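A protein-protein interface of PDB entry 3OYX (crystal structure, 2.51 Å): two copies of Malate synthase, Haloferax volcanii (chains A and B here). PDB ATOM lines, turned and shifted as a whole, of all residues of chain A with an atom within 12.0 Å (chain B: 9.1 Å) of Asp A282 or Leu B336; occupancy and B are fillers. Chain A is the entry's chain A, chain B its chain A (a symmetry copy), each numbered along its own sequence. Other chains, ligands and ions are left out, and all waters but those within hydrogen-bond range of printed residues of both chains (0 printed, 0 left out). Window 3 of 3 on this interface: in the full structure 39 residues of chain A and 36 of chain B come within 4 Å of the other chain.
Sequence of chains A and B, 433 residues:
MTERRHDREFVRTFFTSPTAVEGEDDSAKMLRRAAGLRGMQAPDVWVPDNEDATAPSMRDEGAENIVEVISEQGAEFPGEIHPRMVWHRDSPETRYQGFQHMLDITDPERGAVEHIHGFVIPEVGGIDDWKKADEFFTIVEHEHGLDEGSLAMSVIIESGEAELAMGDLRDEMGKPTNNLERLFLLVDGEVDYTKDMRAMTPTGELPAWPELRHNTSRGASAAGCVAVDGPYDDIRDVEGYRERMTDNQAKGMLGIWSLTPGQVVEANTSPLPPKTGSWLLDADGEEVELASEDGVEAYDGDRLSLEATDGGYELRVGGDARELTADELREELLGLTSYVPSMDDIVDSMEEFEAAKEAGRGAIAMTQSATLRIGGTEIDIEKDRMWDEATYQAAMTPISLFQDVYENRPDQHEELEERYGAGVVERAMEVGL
The backbone carbonyl oxygen (O) of Leu B333 sits at hydrogen-bond distance from the side-chain hydroxyl (OG1) of Thr B337 (3.3 Å).
The backbone NH of Leu A280 is in hydrogen-bond range of the backbone carbonyl oxygen of Ser B338 (3.0 Å). The backbone NH of Asp A282 lies within hydrogen-bond range of the backbone carbonyl oxygen of Leu B336 (2.8 Å).
Along chain A the printed residues that touch a printed residue of chain B span positions 278 to 282. Of the 13 printed residues of chain B, 4 touch a printed residue of chain A. Hydrophobic or aromatic side chains of chain B that line the printed part of chain A: Leu B336 and Tyr B339. Among the printed residues, 9 pairs touch across the chains.
Ser A278 touches Tyr B339 (O to CD1, 3.1 Å). Trp A279 touches Thr B337 (CZ3 to OG1, 3.3 Å). Trp A279 touches Ser B338. CD1 of Tyr B339 touches NE1 of Trp A279 (3.6 Å). Leu A280 touches Leu B336 (O to O, 3.8 Å). Leu A280 touches Thr B337 (O to CA, 3.2 Å). CA of Leu A281 touches O of Leu B336 (3.3 Å).
No position is printed for both chains. Of the 9 pairs that touch across the chains among the printed residues, none has its exchanged pair printed and touching as well.
Of the printed residues of chain B, Ser A278 touches Tyr B339 (3.1 Å). Of the printed residues of chain B, Trp A279 touches Thr B337, Ser B338 and Tyr B339. Of the printed residues of chain B, Leu A280 touches Leu B336 (3.8 Å), Thr B337 (3.2 Å) and Ser B338 (3.0 Å). Leu A281 touches one residue of chain B. No residue of chain B comes within 4 Å of Ala A283. No residue of chain A comes within 4 Å of Glu B332. Gly B335 touches none of the printed residues of chain A. Leu B336 touches just these residues of chain A: Leu A280 (3.8 Å), Leu A281 (3.3 Å) and Asp A282 (2.8 Å). Of the printed residues of chain A, Thr B337 touches Trp A279 (3.3 Å) and Leu A280 (3.2 Å). Of chain A, only Trp A279 and Leu A280 come within 4 Å of Ser B338. Of the printed residues of chain A, Tyr B339 touches Ser A278 and Trp A279. The nearest residue of chain B that does not touch Asp A282 is Gly B335 (4.1 Å). The nearest residue of chain A that does not touch Leu B336 is Ala A283 (4.7 Å).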
ATOM      1  N   SER A 278     -22.427 -18.305  30.102  1.00  0.00           N
ATOM      2  CA  SER A 278     -21.126 -17.659  29.961  1.00  0.00           C
ATOM      3  C   SER A 278     -20.186 -18.809  29.711  1.00  0.00           C
ATOM      4  O   SER A 278     -20.417 -19.910  30.207  1.00  0.00           O
ATOM      5  CB  SER A 278     -20.695 -16.903  31.221  1.00  0.00           C
ATOM      6  OG  SER A 278     -21.318 -15.624  31.297  1.00  0.00           O
ATOM      7  N   TRP A 279     -19.157 -18.569  28.908  1.00  0.00           N
ATOM      8  CA  TRP A 279     -18.168 -19.595  28.578  1.00  0.00           C
ATOM      9  C   TRP A 279     -16.799 -19.129  29.041  1.00  0.00           C
ATOM     10  O   TRP A 279     -16.361 -18.009  28.730  1.00  0.00           O
ATOM     11  CB  TRP A 279     -18.138 -19.898  27.071  1.00  0.00           C
ATOM     12  CG  TRP A 279     -19.120 -20.958  26.585  1.00  0.00           C
ATOM     13  CD1 TRP A 279     -20.400 -20.761  26.111  1.00  0.00           C
ATOM     14  CD2 TRP A 279     -18.877 -22.365  26.502  1.00  0.00           C
ATOM     15  NE1 TRP A 279     -20.960 -21.965  25.753  1.00  0.00           N
ATOM     16  CE2 TRP A 279     -20.047 -22.961  25.975  1.00  0.00           C
ATOM     17  CE3 TRP A 279     -17.785 -23.185  26.838  1.00  0.00           C
ATOM     18  CZ2 TRP A 279     -20.156 -24.341  25.772  1.00  0.00           C
ATOM     19  CZ3 TRP A 279     -17.885 -24.557  26.638  1.00  0.00           C
ATOM     20  CH2 TRP A 279     -19.068 -25.125  26.107  1.00  0.00           C
ATOM     21  N   LEU A 280     -16.136 -19.997  29.791  1.00  0.00           N
ATOM     22  CA  LEU A 280     -14.841 -19.669  30.335  1.00  0.00           C
ATOM     23  C   LEU A 280     -13.829 -20.592  29.691  1.00  0.00           C
ATOM     24  O   LEU A 280     -14.154 -21.741  29.392  1.00  0.00           O
ATOM     25  CB  LEU A 280     -14.871 -19.805  31.857  1.00  0.00           C
ATOM     26  CG  LEU A 280     -16.138 -19.197  32.470  1.00  0.00           C
ATOM     27  CD1 LEU A 280     -16.361 -19.708  33.888  1.00  0.00           C
ATOM     28  CD2 LEU A 280     -16.087 -17.678  32.428  1.00  0.00           C
ATOM     29  N   LEU A 281     -12.627 -20.068  29.446  1.00  0.00           N
ATOM     30  CA  LEU A 281     -11.573 -20.780  28.714  1.00  0.00           C
ATOM     31  C   LEU A 281     -10.246 -20.701  29.480  1.00  0.00           C
ATOM     32  O   LEU A 281      -9.910 -19.653  30.039  1.00  0.00           O
ATOM     33  CB  LEU A 281     -11.434 -20.217  27.282  1.00  0.00           C
ATOM     34  CG  LEU A 281     -10.205 -20.529  26.403  1.00  0.00           C
ATOM     35  CD1 LEU A 281     -10.377 -21.836  25.643  1.00  0.00           C
ATOM     36  CD2 LEU A 281      -9.820 -19.373  25.454  1.00  0.00           C
ATOM     37  N   ASP A 282      -9.487 -21.795  29.452  1.00  0.00           N
ATOM     38  CA  ASP A 282      -8.358 -22.049  30.351  1.00  0.00           C
ATOM     39  C   ASP A 282      -7.207 -21.018  30.381  1.00  0.00           C
ATOM     40  O   ASP A 282      -6.955 -20.450  31.452  1.00  0.00           O
ATOM     41  CB  ASP A 282      -7.832 -23.474  30.133  1.00  0.00           C
ATOM     42  CG  ASP A 282      -7.183 -24.073  31.382  1.00  0.00           C
ATOM     43  OD1 ASP A 282      -6.230 -23.462  31.918  1.00  0.00           O
ATOM     44  OD2 ASP A 282      -7.607 -25.175  31.809  1.00  0.00           O
ATOM     45  N   ALA A 283      -6.503 -20.788  29.265  1.00  0.00           N
ATOM     46  CA  ALA A 283      -5.357 -19.862  29.268  1.00  0.00           C
ATOM     47  C   ALA A 283      -5.399 -18.902  28.094  1.00  0.00           C
ATOM     48  O   ALA A 283      -5.052 -17.730  28.247  1.00  0.00           O
ATOM     49  CB  ALA A 283      -3.978 -20.596  29.346  1.00  0.00           C
ATOM     50  N   ASP B 234     -15.286 -35.947  35.923  1.00  0.00           N
ATOM     51  CA  ASP B 234     -14.774 -35.561  34.648  1.00  0.00           C
ATOM     52  C   ASP B 234     -13.638 -36.545  34.323  1.00  0.00           C
ATOM     53  O   ASP B 234     -12.466 -36.311  34.648  1.00  0.00           O
ATOM     54  CB  ASP B 234     -14.342 -34.104  34.739  1.00  0.00           C
ATOM     55  CG  ASP B 234     -13.964 -33.508  33.396  1.00  0.00           C
ATOM     56  OD1 ASP B 234     -13.376 -32.400  33.444  1.00  0.00           O
ATOM     57  OD2 ASP B 234     -14.229 -34.121  32.321  1.00  0.00           O
ATOM     58  N   ASP B 237     -10.567 -35.896  31.986  1.00  0.00           N
ATOM     59  CA  ASP B 237      -9.626 -34.961  32.591  1.00  0.00           C
ATOM     60  C   ASP B 237      -8.605 -35.758  33.380  1.00  0.00           C
ATOM     61  O   ASP B 237      -8.549 -35.673  34.591  1.00  0.00           O
ATOM     62  CB  ASP B 237     -10.384 -33.931  33.449  1.00  0.00           C
ATOM     63  CG  ASP B 237      -9.470 -32.932  34.155  1.00  0.00           C
ATOM     64  OD1 ASP B 237      -8.262 -32.884  33.864  1.00  0.00           O
ATOM     65  OD2 ASP B 237      -9.969 -32.180  35.018  1.00  0.00           O
ATOM     66  N   GLU B 239      -5.382 -35.350  33.754  1.00  0.00           N
ATOM     67  CA  GLU B 239      -4.327 -34.617  34.464  1.00  0.00           C
ATOM     68  C   GLU B 239      -4.838 -34.046  35.804  1.00  0.00           C
ATOM     69  O   GLU B 239      -4.111 -34.075  36.801  1.00  0.00           O
ATOM     70  CB  GLU B 239      -3.717 -33.532  33.550  1.00  0.00           C
ATOM     71  CG  GLU B 239      -2.838 -32.467  34.242  1.00  0.00           C
ATOM     72  CD  GLU B 239      -1.460 -32.975  34.754  1.00  0.00           C
ATOM     73  OE1 GLU B 239      -0.950 -34.031  34.276  1.00  0.00           O
ATOM     74  OE2 GLU B 239      -0.873 -32.287  35.646  1.00  0.00           O
ATOM     75  N   GLU B 243      -3.629 -34.503  39.562  1.00  0.00           N
ATOM     76  CA  GLU B 243      -3.455 -33.393  40.493  1.00  0.00           C
ATOM     77  C   GLU B 243      -4.217 -33.633  41.827  1.00  0.00           C
ATOM     78  O   GLU B 243      -3.664 -33.471  42.919  1.00  0.00           O
ATOM     79  CB  GLU B 243      -3.868 -32.059  39.849  1.00  0.00           C
ATOM     80  CG  GLU B 243      -2.698 -31.390  39.115  1.00  0.00           C
ATOM     81  CD  GLU B 243      -3.111 -30.435  37.979  1.00  0.00           C
ATOM     82  OE1 GLU B 243      -4.331 -30.327  37.654  1.00  0.00           O
ATOM     83  OE2 GLU B 243      -2.193 -29.788  37.408  1.00  0.00           O
ATOM     84  N   GLU B 331     -11.683 -29.758  18.969  1.00  0.00           N
ATOM     85  CA  GLU B 331     -12.415 -30.661  19.857  1.00  0.00           C
ATOM     86  C   GLU B 331     -11.722 -30.863  21.222  1.00  0.00           C
ATOM     87  O   GLU B 331     -12.389 -30.897  22.253  1.00  0.00           O
ATOM     88  CB  GLU B 331     -12.699 -32.008  19.166  1.00  0.00           C
ATOM     89  CG  GLU B 331     -13.668 -32.935  19.937  1.00  0.00           C
ATOM     90  CD  GLU B 331     -13.373 -34.444  19.809  1.00  0.00           C
ATOM     91  OE1 GLU B 331     -12.301 -34.840  19.283  1.00  0.00           O
ATOM     92  OE2 GLU B 331     -14.225 -35.246  20.262  1.00  0.00           O
ATOM     93  N   GLU B 332     -10.394 -30.995  21.234  1.00  0.00           N
ATOM     94  CA  GLU B 332      -9.612 -31.098  22.485  1.00  0.00           C
ATOM     95  C   GLU B 332      -9.782 -29.849  23.396  1.00  0.00           C
ATOM     96  O   GLU B 332      -9.278 -29.800  24.526  1.00  0.00           O
ATOM     97  CB  GLU B 332      -8.135 -31.403  22.141  1.00  0.00           C
ATOM     98  CG  GLU B 332      -7.163 -31.550  23.321  1.00  0.00           C
ATOM     99  CD  GLU B 332      -6.350 -30.282  23.594  1.00  0.00           C
ATOM    100  OE1 GLU B 332      -6.909 -29.165  23.541  1.00  0.00           O
ATOM    101  OE2 GLU B 332      -5.137 -30.395  23.870  1.00  0.00           O
ATOM    102  N   LEU B 333     -10.511 -28.853  22.887  1.00  0.00           N
ATOM    103  CA  LEU B 333     -10.876 -27.616  23.596  1.00  0.00           C
ATOM    104  C   LEU B 333     -11.795 -27.799  24.819  1.00  0.00           C
ATOM    105  O   LEU B 333     -11.892 -26.902  25.672  1.00  0.00           O
ATOM    106  CB  LEU B 333     -11.544 -26.636  22.609  1.00  0.00           C
ATOM    107  CG  LEU B 333     -10.882 -25.278  22.325  1.00  0.00           C
ATOM    108  CD1 LEU B 333      -9.383 -25.411  22.071  1.00  0.00           C
ATOM    109  CD2 LEU B 333     -11.604 -24.524  21.197  1.00  0.00           C
ATOM    110  N   LEU B 334     -12.469 -28.947  24.897  1.00  0.00           N
ATOM    111  CA  LEU B 334     -13.423 -29.220  25.970  1.00  0.00           C
ATOM    112  C   LEU B 334     -12.795 -29.254  27.378  1.00  0.00           C
ATOM    113  O   LEU B 334     -13.412 -28.831  28.358  1.00  0.00           O
ATOM    114  CB  LEU B 334     -14.227 -30.492  25.666  1.00  0.00           C
ATOM    115  CG  LEU B 334     -15.048 -30.619  24.368  1.00  0.00           C
ATOM    116  CD1 LEU B 334     -15.829 -31.942  24.346  1.00  0.00           C
ATOM    117  CD2 LEU B 334     -15.978 -29.425  24.059  1.00  0.00           C
ATOM    118  N   GLY B 335     -11.562 -29.742  27.468  1.00  0.00           N
ATOM    119  CA  GLY B 335     -10.832 -29.785  28.732  1.00  0.00           C
ATOM    120  C   GLY B 335     -10.174 -28.459  29.038  1.00  0.00           C
ATOM    121  O   GLY B 335      -9.357 -28.358  29.967  1.00  0.00           O
ATOM    122  N   LEU B 336     -10.525 -27.457  28.228  1.00  0.00           N
ATOM    123  CA  LEU B 336     -10.102 -26.070  28.418  1.00  0.00           C
ATOM    124  C   LEU B 336     -11.298 -25.135  28.579  1.00  0.00           C
ATOM    125  O   LEU B 336     -11.147 -24.014  29.040  1.00  0.00           O
ATOM    126  CB  LEU B 336      -9.195 -25.596  27.275  1.00  0.00           C
ATOM    127  CG  LEU B 336      -7.708 -25.969  27.408  1.00  0.00           C
ATOM    128  CD1 LEU B 336      -7.401 -27.357  26.787  1.00  0.00           C
ATOM    129  CD2 LEU B 336      -6.753 -24.878  26.866  1.00  0.00           C
ATOM    130  N   THR B 337     -12.491 -25.580  28.209  1.00  0.00           N
ATOM    131  CA  THR B 337     -13.681 -24.791  28.502  1.00  0.00           C
ATOM    132  C   THR B 337     -14.528 -25.335  29.646  1.00  0.00           C
ATOM    133  O   THR B 337     -14.477 -26.524  29.996  1.00  0.00           O
ATOM    134  CB  THR B 337     -14.622 -24.627  27.298  1.00  0.00           C
ATOM    135  OG1 THR B 337     -14.881 -25.903  26.703  1.00  0.00           O
ATOM    136  CG2 THR B 337     -14.012 -23.699  26.291  1.00  0.00           C
ATOM    137  N   SER B 338     -15.317 -24.425  30.209  1.00  0.00           N
ATOM    138  CA  SER B 338     -16.382 -24.748  31.153  1.00  0.00           C
ATOM    139  C   SER B 338     -17.518 -23.753  30.945  1.00  0.00           C
ATOM    140  O   SER B 338     -17.341 -22.668  30.377  1.00  0.00           O
ATOM    141  CB  SER B 338     -15.873 -24.725  32.597  1.00  0.00           C
ATOM    142  OG  SER B 338     -15.209 -23.499  32.848  1.00  0.00           O
ATOM    143  N   TYR B 339     -18.688 -24.147  31.418  1.00  0.00           N
ATOM    144  CA  TYR B 339     -19.904 -23.431  31.158  1.00  0.00           C
ATOM    145  C   TYR B 339     -20.643 -23.109  32.462  1.00  0.00           C
ATOM    146  O   TYR B 339     -21.067 -24.036  33.164  1.00  0.00           O
ATOM    147  CB  TYR B 339     -20.798 -24.326  30.302  1.00  0.00           C
ATOM    148  CG  TYR B 339     -22.053 -23.621  29.909  1.00  0.00           C
ATOM    149  CD1 TYR B 339     -21.968 -22.439  29.198  1.00  0.00           C
ATOM    150  CD2 TYR B 339     -23.304 -24.100  30.264  1.00  0.00           C
ATOM    151  CE1 TYR B 339     -23.072 -21.752  28.824  1.00  0.00           C
ATOM    152  CE2 TYR B 339     -24.456 -23.401  29.877  1.00  0.00           C
ATOM    153  CZ  TYR B 339     -24.309 -22.226  29.157  1.00  0.00           C
ATOM    154  OH  TYR B 339     -25.348 -21.446  28.754  1.00  0.00           O
